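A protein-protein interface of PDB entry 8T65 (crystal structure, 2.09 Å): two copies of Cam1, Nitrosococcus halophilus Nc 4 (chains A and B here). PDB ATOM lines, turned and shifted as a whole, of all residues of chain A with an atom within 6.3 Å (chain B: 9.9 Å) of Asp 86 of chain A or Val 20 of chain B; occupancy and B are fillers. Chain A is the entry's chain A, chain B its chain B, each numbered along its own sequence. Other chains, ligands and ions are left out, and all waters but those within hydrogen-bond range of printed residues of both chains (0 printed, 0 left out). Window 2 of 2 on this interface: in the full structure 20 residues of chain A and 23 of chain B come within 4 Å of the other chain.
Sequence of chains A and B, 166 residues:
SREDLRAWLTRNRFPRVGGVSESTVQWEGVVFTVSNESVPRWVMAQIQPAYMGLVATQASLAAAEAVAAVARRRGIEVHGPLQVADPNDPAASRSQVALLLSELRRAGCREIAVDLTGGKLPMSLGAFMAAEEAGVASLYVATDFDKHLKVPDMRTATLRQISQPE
O of Ile 162 of chain B is in hydrogen-bond range of N of Gly 18 of chain B (3.4 Å). N of Ala 92 of chain A is in hydrogen-bond range of OD2 of Asp 89 of chain A, at 3.4 Å. The side-chain hydroxyl (OG1) of Thr 158 of chain B sits at hydrogen-bond distance from the guanidinium group (NE) of Arg 160 of chain B (2.6 Å). The backbone NH (N) of Ala 142 of chain B lies within hydrogen-bond range of the backbone carbonyl oxygen (O) of Thr 158 of chain B, 2.9 Å away. The side-chain carboxylate of Asp 86 of chain A sits close to the backbone NH of Asn 88 of chain A, at 3.2 Å. The backbone carbonyl oxygen of Tyr 140 of chain B is in hydrogen-bond range of the backbone NH of Arg 160 of chain B (2.6 Å).
No position is printed for both chains. Of the 8 pairs that touch across the chains among the printed residues, none has its exchanged pair printed and touching as well.
O of Gly 18 of chain B sits close to OD1 of Asp 89 of chain A (2.7 Å). The side-chain carboxylate (OD1) of Asp 89 of chain A lies close to the backbone carbonyl oxygen (O) of Gly 19 of chain B, at 3.3 Å.
Of the 22 printed residues of chain B, 7 touch a printed residue of chain A. Printed residues of chain B that touch a printed residue of chain A: Val 17, Gly 18, Gly 19, Val 20, Tyr 140, Ala 142 and Arg 160. Hydrophobic or aromatic side chains of chain B that line the printed part of chain A: Val 17, Val 20, Tyr 140 and Ala 142. Hydrophobic or aromatic side chains of chain A that line the printed part of chain B: Pro 90. Among the printed residues, 8 pairs touch across the chains. Among the printed residues, no Asp or Glu carboxylate lies within 4 Å of a Lys or Arg side-chain nitrogen of the other chain.
No residue of chain B comes within 4 Å of Val 84 of chain A. No residue of chain B comes within 4 Å of Ala 85 of chain A. Asp 86 of chain A touches just one residue of chain B: Val 20 (3.1 Å). Asn 88 of chain A touches three residues of chain B. Of the printed residues of chain A, Val 17 of chain B touches Pro 90 (3.5 Å). Of the printed residues of chain A, Gly 18 of chain B touches Asp 89 and Pro 90. Val 20 of chain B touches just one residue of chain A: Asp 86. Of the printed residues of chain A, Arg 160 of chain B touches Asn 88 (3.6 Å). The nearest residue of chain B that does not touch Asp 86 of chain A is Arg 160 of chain B (4.6 Å). The nearest residue of chain A that does not touch Val 20 of chain B is Asp 89 of chain A (4.1 Å).
Asp 86 of chain A touches Val 20 of chain B (OD2 to CG2, 3.1 Å). OD1 of Asn 88 of chain A touches CE2 of Tyr 140 of chain B (3.8 Å). OD1 of Asn 88 of chain A touches CB of Ala 142 of chain B, at 3.3 Å. Asn 88 of chain A touches Arg 160 of chain B. Val 17 of chain B touches Pro 90 of chain A (CG1 to CG, 3.5 Å). O of Gly 18 of chain B touches CD of Pro 90 of chain A, 3.8 Å away.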
ATOM      1  N   THR A  57     -12.903 -11.922  -6.239  1.00  0.00           N
ATOM      2  CA  THR A  57     -12.258 -13.221  -6.248  1.00  0.00           C
ATOM      3  C   THR A  57     -12.394 -13.834  -4.864  1.00  0.00           C
ATOM      4  O   THR A  57     -12.877 -13.202  -3.923  1.00  0.00           O
ATOM      5  CB  THR A  57     -10.773 -13.110  -6.604  1.00  0.00           C
ATOM      6  OG1 THR A  57     -10.064 -12.518  -5.503  1.00  0.00           O
ATOM      7  CG2 THR A  57     -10.586 -12.238  -7.840  1.00  0.00           C
ATOM      8  N   VAL A  84     -14.979 -14.531  -9.529  1.00  0.00           N
ATOM      9  CA  VAL A  84     -14.286 -15.098 -10.677  1.00  0.00           C
ATOM     10  C   VAL A  84     -13.366 -16.201 -10.166  1.00  0.00           C
ATOM     11  O   VAL A  84     -12.691 -16.042  -9.144  1.00  0.00           O
ATOM     12  CB  VAL A  84     -13.519 -14.026 -11.477  1.00  0.00           C
ATOM     13  CG1 VAL A  84     -14.468 -12.895 -11.852  1.00  0.00           C
ATOM     14  CG2 VAL A  84     -12.326 -13.472 -10.698  1.00  0.00           C
ATOM     15  N   ALA A  85     -13.366 -17.340 -10.855  1.00  0.00           N
ATOM     16  CA  ALA A  85     -12.469 -18.421 -10.463  1.00  0.00           C
ATOM     17  C   ALA A  85     -11.001 -18.049 -10.659  1.00  0.00           C
ATOM     18  O   ALA A  85     -10.149 -18.489  -9.875  1.00  0.00           O
ATOM     19  CB  ALA A  85     -12.792 -19.686 -11.254  1.00  0.00           C
ATOM     20  N   ASP A  86     -10.678 -17.258 -11.681  1.00  0.00           N
ATOM     21  CA  ASP A  86      -9.284 -16.913 -11.987  1.00  0.00           C
ATOM     22  C   ASP A  86      -9.147 -15.424 -12.261  1.00  0.00           C
ATOM     23  O   ASP A  86      -9.599 -14.950 -13.323  1.00  0.00           O
ATOM     24  CB  ASP A  86      -8.748 -17.698 -13.178  1.00  0.00           C
ATOM     25  CG  ASP A  86      -7.301 -17.329 -13.520  1.00  0.00           C
ATOM     26  OD1 ASP A  86      -6.519 -16.962 -12.610  1.00  0.00           O
ATOM     27  OD2 ASP A  86      -6.953 -17.362 -14.713  1.00  0.00           O
ATOM     28  N   PRO A  87      -8.507 -14.668 -11.367  1.00  0.00           N
ATOM     29  CA  PRO A  87      -8.373 -13.223 -11.595  1.00  0.00           C
ATOM     30  C   PRO A  87      -7.416 -12.867 -12.722  1.00  0.00           C
ATOM     31  O   PRO A  87      -7.348 -11.689 -13.110  1.00  0.00           O
ATOM     32  CB  PRO A  87      -7.871 -12.698 -10.246  1.00  0.00           C
ATOM     33  CG  PRO A  87      -7.205 -13.875  -9.604  1.00  0.00           C
ATOM     34  CD  PRO A  87      -7.900 -15.103 -10.097  1.00  0.00           C
ATOM     35  N   ASN A  88      -6.676 -13.827 -13.268  1.00  0.00           N
ATOM     36  CA  ASN A  88      -5.758 -13.529 -14.360  1.00  0.00           C
ATOM     37  C   ASN A  88      -6.414 -13.670 -15.723  1.00  0.00           C
ATOM     38  O   ASN A  88      -5.769 -13.392 -16.735  1.00  0.00           O
ATOM     39  CB  ASN A  88      -4.534 -14.438 -14.272  1.00  0.00           C
ATOM     40  CG  ASN A  88      -3.786 -14.249 -12.985  1.00  0.00           C
ATOM     41  OD1 ASN A  88      -3.455 -13.126 -12.604  1.00  0.00           O
ATOM     42  ND2 ASN A  88      -3.542 -15.344 -12.285  1.00  0.00           N
ATOM     43  N   ASP A  89      -7.681 -14.069 -15.757  1.00  0.00           N
ATOM     44  CA  ASP A  89      -8.405 -14.358 -16.990  1.00  0.00           C
ATOM     45  C   ASP A  89      -9.395 -13.242 -17.288  1.00  0.00           C
ATOM     46  O   ASP A  89     -10.457 -13.181 -16.650  1.00  0.00           O
ATOM     47  CB  ASP A  89      -9.134 -15.701 -16.857  1.00  0.00           C
ATOM     48  CG  ASP A  89      -9.909 -16.073 -18.105  1.00  0.00           C
ATOM     49  OD1 ASP A  89      -9.622 -15.503 -19.187  1.00  0.00           O
ATOM     50  OD2 ASP A  89     -10.809 -16.935 -18.002  1.00  0.00           O
ATOM     51  N   PRO A  90      -9.114 -12.359 -18.251  1.00  0.00           N
ATOM     52  CA  PRO A  90     -10.078 -11.287 -18.549  1.00  0.00           C
ATOM     53  C   PRO A  90     -11.412 -11.813 -19.040  1.00  0.00           C
ATOM     54  O   PRO A  90     -12.435 -11.154 -18.833  1.00  0.00           O
ATOM     55  CB  PRO A  90      -9.360 -10.450 -19.616  1.00  0.00           C
ATOM     56  CG  PRO A  90      -8.342 -11.374 -20.208  1.00  0.00           C
ATOM     57  CD  PRO A  90      -7.934 -12.322 -19.135  1.00  0.00           C
ATOM     58  N   ALA A  92     -13.023 -14.350 -17.852  1.00  0.00           N
ATOM     59  CA  ALA A  92     -13.817 -14.727 -16.687  1.00  0.00           C
ATOM     60  C   ALA A  92     -14.455 -13.505 -16.031  1.00  0.00           C
ATOM     61  O   ALA A  92     -15.601 -13.568 -15.565  1.00  0.00           O
ATOM     62  CB  ALA A  92     -12.941 -15.477 -15.687  1.00  0.00           C
ATOM     63  N   SER A  93     -13.725 -12.386 -15.991  1.00  0.00           N
ATOM     64  CA  SER A  93     -14.268 -11.145 -15.452  1.00  0.00           C
ATOM     65  C   SER A  93     -15.280 -10.518 -16.408  1.00  0.00           C
ATOM     66  O   SER A  93     -16.247  -9.889 -15.964  1.00  0.00           O
ATOM     67  CB  SER A  93     -13.137 -10.161 -15.177  1.00  0.00           C
ATOM     68  OG  SER A  93     -12.470 -10.521 -13.976  1.00  0.00           O
ATOM     69  N   MET A 123      -8.827  -8.413 -14.599  1.00  0.00           N
ATOM     70  CA  MET A 123     -10.190  -8.136 -14.150  1.00  0.00           C
ATOM     71  C   MET A 123     -10.683  -6.801 -14.694  1.00  0.00           C
ATOM     72  O   MET A 123     -11.817  -6.698 -15.185  1.00  0.00           O
ATOM     73  CB  MET A 123     -10.259  -8.148 -12.619  1.00  0.00           C
ATOM     74  CG  MET A 123      -9.955  -9.506 -11.987  1.00  0.00           C
ATOM     75  SD  MET A 123      -9.829  -9.470 -10.176  1.00  0.00           S
ATOM     76  CE  MET A 123     -11.566  -9.316  -9.730  1.00  0.00           C
ATOM     77  N   ARG B  16      -8.356 -11.719 -30.321  1.00  0.00           N
ATOM     78  CA  ARG B  16      -9.448 -12.095 -29.436  1.00  0.00           C
ATOM     79  C   ARG B  16      -8.937 -12.277 -28.015  1.00  0.00           C
ATOM     80  O   ARG B  16      -7.857 -12.836 -27.802  1.00  0.00           O
ATOM     81  CB  ARG B  16     -10.135 -13.362 -29.937  1.00  0.00           C
ATOM     82  CG  ARG B  16     -11.268 -13.040 -30.893  1.00  0.00           C
ATOM     83  CD  ARG B  16     -12.262 -12.138 -30.190  1.00  0.00           C
ATOM     84  NE  ARG B  16     -12.696 -12.748 -28.935  1.00  0.00           N
ATOM     85  CZ  ARG B  16     -12.918 -12.087 -27.801  1.00  0.00           C
ATOM     86  NH1 ARG B  16     -13.318 -12.753 -26.719  1.00  0.00           N
ATOM     87  NH2 ARG B  16     -12.738 -10.769 -27.744  1.00  0.00           N
ATOM     88  N   VAL B  17      -9.711 -11.779 -27.052  1.00  0.00           N
ATOM     89  CA  VAL B  17      -9.316 -11.763 -25.646  1.00  0.00           C
ATOM     90  C   VAL B  17      -9.826 -13.031 -24.982  1.00  0.00           C
ATOM     91  O   VAL B  17     -11.037 -13.283 -24.948  1.00  0.00           O
ATOM     92  CB  VAL B  17      -9.848 -10.517 -24.929  1.00  0.00           C
ATOM     93  CG1 VAL B  17      -9.459 -10.567 -23.464  1.00  0.00           C
ATOM     94  CG2 VAL B  17      -9.315  -9.260 -25.606  1.00  0.00           C
ATOM     95  N   GLY B  18      -8.907 -13.815 -24.431  1.00  0.00           N
ATOM     96  CA  GLY B  18      -9.229 -15.179 -24.078  1.00  0.00           C
ATOM     97  C   GLY B  18      -8.938 -15.558 -22.646  1.00  0.00           C
ATOM     98  O   GLY B  18      -9.223 -14.788 -21.724  1.00  0.00           O
ATOM     99  N   GLY B  19      -8.348 -16.742 -22.458  1.00  0.00           N
ATOM    100  CA  GLY B  19      -8.229 -17.364 -21.152  1.00  0.00           C
ATOM    101  C   GLY B  19      -6.924 -17.196 -20.393  1.00  0.00           C
ATOM    102  O   GLY B  19      -6.483 -16.075 -20.129  1.00  0.00           O
ATOM    103  N   VAL B  20      -6.306 -18.322 -20.029  1.00  0.00           N
ATOM    104  CA  VAL B  20      -5.260 -18.357 -19.008  1.00  0.00           C
ATOM    105  C   VAL B  20      -3.880 -18.620 -19.585  1.00  0.00           C
ATOM    106  O   VAL B  20      -2.878 -18.348 -18.900  1.00  0.00           O
ATOM    107  CB  VAL B  20      -5.594 -19.408 -17.921  1.00  0.00           C
ATOM    108  CG1 VAL B  20      -4.486 -19.547 -16.864  1.00  0.00           C
ATOM    109  CG2 VAL B  20      -6.931 -19.089 -17.272  1.00  0.00           C
ATOM    110  N   SER B  21      -3.790 -19.093 -20.824  1.00  0.00           N
ATOM    111  CA  SER B  21      -2.547 -19.641 -21.356  1.00  0.00           C
ATOM    112  C   SER B  21      -1.366 -18.701 -21.145  1.00  0.00           C
ATOM    113  O   SER B  21      -1.491 -17.481 -21.275  1.00  0.00           O
ATOM    114  CB  SER B  21      -2.710 -19.944 -22.845  1.00  0.00           C
ATOM    115  OG  SER B  21      -2.496 -18.774 -23.618  1.00  0.00           O
ATOM    116  N   GLU B  22      -0.226 -19.286 -20.781  1.00  0.00           N
ATOM    117  CA  GLU B  22       1.030 -18.554 -20.726  1.00  0.00           C
ATOM    118  C   GLU B  22       1.474 -18.220 -22.139  1.00  0.00           C
ATOM    119  O   GLU B  22       1.265 -19.003 -23.066  1.00  0.00           O
ATOM    120  CB  GLU B  22       2.105 -19.395 -20.028  1.00  0.00           C
ATOM    121  CG  GLU B  22       1.608 -20.067 -18.741  1.00  0.00           C
ATOM    122  CD  GLU B  22       2.730 -20.431 -17.785  1.00  0.00           C
ATOM    123  OE1 GLU B  22       3.856 -20.734 -18.250  1.00  0.00           O
ATOM    124  OE2 GLU B  22       2.481 -20.418 -16.561  1.00  0.00           O
ATOM    125  N   SER B  23       2.084 -17.054 -22.309  1.00  0.00           N
ATOM    126  CA  SER B  23       2.662 -16.726 -23.605  1.00  0.00           C
ATOM    127  C   SER B  23       3.977 -17.475 -23.749  1.00  0.00           C
ATOM    128  O   SER B  23       4.885 -17.310 -22.929  1.00  0.00           O
ATOM    129  CB  SER B  23       2.898 -15.228 -23.755  1.00  0.00           C
ATOM    130  OG  SER B  23       3.326 -14.952 -25.079  1.00  0.00           O
ATOM    131  N   THR B  24       4.096 -18.284 -24.799  1.00  0.00           N
ATOM    132  CA  THR B  24       5.274 -19.124 -24.965  1.00  0.00           C
ATOM    133  C   THR B  24       6.049 -18.793 -26.235  1.00  0.00           C
ATOM    134  O   THR B  24       6.876 -19.596 -26.672  1.00  0.00           O
ATOM    135  CB  THR B  24       4.867 -20.596 -24.945  1.00  0.00           C
ATOM    136  OG1 THR B  24       3.851 -20.813 -25.933  1.00  0.00           O
ATOM    137  CG2 THR B  24       4.309 -20.975 -23.562  1.00  0.00           C
ATOM    138  N   SER B 138      -1.236  -9.114 -26.745  1.00  0.00           N
ATOM    139  CA  SER B 138      -1.032  -8.408 -25.489  1.00  0.00           C
ATOM    140  C   SER B 138      -0.606  -9.411 -24.429  1.00  0.00           C
ATOM    141  O   SER B 138      -1.174 -10.508 -24.350  1.00  0.00           O
ATOM    142  CB  SER B 138      -2.334  -7.705 -25.020  1.00  0.00           C
ATOM    143  OG  SER B 138      -2.618  -6.555 -25.800  1.00  0.00           O
ATOM    144  N   TYR B 140       0.774 -10.075 -20.134  1.00  0.00           N
ATOM    145  CA  TYR B 140       0.609  -9.636 -18.760  1.00  0.00           C
ATOM    146  C   TYR B 140       1.463 -10.540 -17.882  1.00  0.00           C
ATOM    147  O   TYR B 140       1.467 -11.761 -18.065  1.00  0.00           O
ATOM    148  CB  TYR B 140      -0.872  -9.704 -18.337  1.00  0.00           C
ATOM    149  CG  TYR B 140      -1.153  -9.517 -16.842  1.00  0.00           C
ATOM    150  CD1 TYR B 140      -0.953  -8.284 -16.233  1.00  0.00           C
ATOM    151  CD2 TYR B 140      -1.642 -10.560 -16.057  1.00  0.00           C
ATOM    152  CE1 TYR B 140      -1.203  -8.094 -14.890  1.00  0.00           C
ATOM    153  CE2 TYR B 140      -1.916 -10.377 -14.705  1.00  0.00           C
ATOM    154  CZ  TYR B 140      -1.699  -9.134 -14.133  1.00  0.00           C
ATOM    155  OH  TYR B 140      -1.947  -8.917 -12.783  1.00  0.00           O
ATOM    156  N   VAL B 141       2.176  -9.949 -16.931  1.00  0.00           N
ATOM    157  CA  VAL B 141       2.912 -10.727 -15.937  1.00  0.00           C
ATOM    158  C   VAL B 141       1.985 -10.928 -14.748  1.00  0.00           C
ATOM    159  O   VAL B 141       1.634  -9.972 -14.049  1.00  0.00           O
ATOM    160  CB  VAL B 141       4.212 -10.033 -15.520  1.00  0.00           C
ATOM    161  CG1 VAL B 141       4.899 -10.827 -14.404  1.00  0.00           C
ATOM    162  CG2 VAL B 141       5.130  -9.867 -16.723  1.00  0.00           C
ATOM    163  N   ALA B 142       1.575 -12.168 -14.519  1.00  0.00           N
ATOM    164  CA  ALA B 142       0.716 -12.500 -13.391  1.00  0.00           C
ATOM    165  C   ALA B 142       1.559 -13.041 -12.241  1.00  0.00           C
ATOM    166  O   ALA B 142       2.415 -13.912 -12.443  1.00  0.00           O
ATOM    167  CB  ALA B 142      -0.353 -13.518 -13.793  1.00  0.00           C
ATOM    168  N   THR B 143       1.330 -12.508 -11.041  1.00  0.00           N
ATOM    169  CA  THR B 143       1.988 -12.979  -9.833  1.00  0.00           C
ATOM    170  C   THR B 143       0.940 -13.215  -8.759  1.00  0.00           C
ATOM    171  O   THR B 143      -0.156 -12.655  -8.807  1.00  0.00           O
ATOM    172  CB  THR B 143       3.032 -11.974  -9.304  1.00  0.00           C
ATOM    173  OG1 THR B 143       2.373 -10.760  -8.908  1.00  0.00           O
ATOM    174  CG2 THR B 143       4.066 -11.658 -10.369  1.00  0.00           C
ATOM    175  N   ASP B 144       1.291 -14.053  -7.786  1.00  0.00           N
ATOM    176  CA  ASP B 144       0.520 -14.169  -6.554  1.00  0.00           C
ATOM    177  C   ASP B 144       0.977 -13.092  -5.576  1.00  0.00           C
ATOM    178  O   ASP B 144       2.123 -12.637  -5.613  1.00  0.00           O
ATOM    179  CB  ASP B 144       0.677 -15.561  -5.932  1.00  0.00           C
ATOM    180  CG  ASP B 144       0.169 -16.674  -6.854  1.00  0.00           C
ATOM    181  OD1 ASP B 144      -0.879 -16.476  -7.506  1.00  0.00           O
ATOM    182  OD2 ASP B 144       0.825 -17.740  -6.935  1.00  0.00           O
ATOM    183  N   THR B 158       4.598 -15.369 -13.785  1.00  0.00           N
ATOM    184  CA  THR B 158       4.445 -16.053 -15.058  1.00  0.00           C
ATOM    185  C   THR B 158       4.016 -15.025 -16.091  1.00  0.00           C
ATOM    186  O   THR B 158       3.385 -14.015 -15.760  1.00  0.00           O
ATOM    187  CB  THR B 158       3.403 -17.203 -15.000  1.00  0.00           C
ATOM    188  OG1 THR B 158       2.140 -16.695 -14.566  1.00  0.00           O
ATOM    189  CG2 THR B 158       3.848 -18.296 -14.032  1.00  0.00           C
ATOM    190  N   LEU B 159       4.357 -15.292 -17.342  1.00  0.00           N
ATOM    191  CA  LEU B 159       4.014 -14.409 -18.450  1.00  0.00           C
ATOM    192  C   LEU B 159       2.764 -14.960 -19.118  1.00  0.00           C
ATOM    193  O   LEU B 159       2.792 -16.054 -19.691  1.00  0.00           O
ATOM    194  CB  LEU B 159       5.177 -14.296 -19.432  1.00  0.00           C
ATOM    195  CG  LEU B 159       5.056 -13.360 -20.635  1.00  0.00           C
ATOM    196  CD1 LEU B 159       4.882 -11.899 -20.209  1.00  0.00           C
ATOM    197  CD2 LEU B 159       6.294 -13.524 -21.496  1.00  0.00           C
ATOM    198  N   ARG B 160       1.667 -14.215 -19.026  1.00  0.00           N
ATOM    199  CA  ARG B 160       0.397 -14.619 -19.600  1.00  0.00           C
ATOM    200  C   ARG B 160       0.142 -13.882 -20.910  1.00  0.00           C
ATOM    201  O   ARG B 160       0.510 -12.711 -21.072  1.00  0.00           O
ATOM    202  CB  ARG B 160      -0.744 -14.348 -18.628  1.00  0.00           C
ATOM    203  CG  ARG B 160      -0.487 -14.866 -17.220  1.00  0.00           C
ATOM    204  CD  ARG B 160      -0.287 -16.384 -17.190  1.00  0.00           C
ATOM    205  NE  ARG B 160      -0.172 -16.883 -15.819  1.00  0.00           N
ATOM    206  CZ  ARG B 160      -1.205 -17.211 -15.051  1.00  0.00           C
ATOM    207  NH1 ARG B 160      -0.997 -17.656 -13.815  1.00  0.00           N
ATOM    208  NH2 ARG B 160      -2.443 -17.108 -15.523  1.00  0.00           N
ATOM    209  N   GLN B 161      -0.470 -14.593 -21.856  1.00  0.00           N
ATOM    210  CA  GLN B 161      -0.937 -14.000 -23.103  1.00  0.00           C
ATOM    211  C   GLN B 161      -2.384 -13.571 -22.907  1.00  0.00           C
ATOM    212  O   GLN B 161      -3.265 -14.412 -22.711  1.00  0.00           O
ATOM    213  CB  GLN B 161      -0.816 -14.975 -24.274  1.00  0.00           C
ATOM    214  CG  GLN B 161      -1.010 -14.254 -25.605  1.00  0.00           C
ATOM    215  CD  GLN B 161      -0.294 -14.905 -26.770  1.00  0.00           C
ATOM    216  OE1 GLN B 161       0.714 -15.587 -26.592  1.00  0.00           O
ATOM    217  NE2 GLN B 161      -0.804 -14.678 -27.981  1.00  0.00           N
ATOM    218  N   ILE B 162      -2.625 -12.259 -22.957  1.00  0.00           N
ATOM    219  CA  ILE B 162      -3.962 -11.712 -22.729  1.00  0.00           C
ATOM    220  C   ILE B 162      -4.855 -11.887 -23.958  1.00  0.00           C
ATOM    221  O   ILE B 162      -6.070 -12.087 -23.827  1.00  0.00           O
ATOM    222  CB  ILE B 162      -3.857 -10.225 -22.328  1.00  0.00           C
ATOM    223  CG1 ILE B 162      -3.336 -10.080 -20.904  1.00  0.00           C
ATOM    224  CG2 ILE B 162      -5.167  -9.504 -22.513  1.00  0.00           C
ATOM    225  CD1 ILE B 162      -4.024 -10.975 -19.897  1.00  0.00           C
ATOM    226  N   SER B 163      -4.291 -11.816 -25.163  1.00  0.00           N
ATOM    227  CA  SER B 163      -5.089 -11.881 -26.379  1.00  0.00           C
ATOM    228  C   SER B 163      -4.387 -12.734 -27.426  1.00  0.00           C
ATOM    229  O   SER B 163      -3.176 -12.964 -27.364  1.00  0.00           O
ATOM    230  CB  SER B 163      -5.348 -10.490 -26.947  1.00  0.00           C
ATOM    231  OG  SER B 163      -4.196 -10.044 -27.636  1.00  0.00           O
ATOM    232  N   GLN B 164      -5.163 -13.180 -28.407  1.00  0.00           N
ATOM    233  CA  GLN B 164      -4.672 -14.089 -29.441  1.00  0.00           C
ATOM    234  C   GLN B 164      -4.843 -13.457 -30.813  1.00  0.00           C
ATOM    235  O   GLN B 164      -5.979 -13.404 -31.324  1.00  0.00           O
ATOM    236  CB  GLN B 164      -5.407 -15.427 -29.377  1.00  0.00           C
ATOM    237  CG  GLN B 164      -4.898 -16.457 -30.379  1.00  0.00           C
ATOM    238  CD  GLN B 164      -3.667 -17.200 -29.873  1.00  0.00           C
ATOM    239  OE1 GLN B 164      -3.717 -17.870 -28.841  1.00  0.00           O
ATOM    240  NE2 GLN B 164      -2.556 -17.078 -30.594  1.00  0.00           N
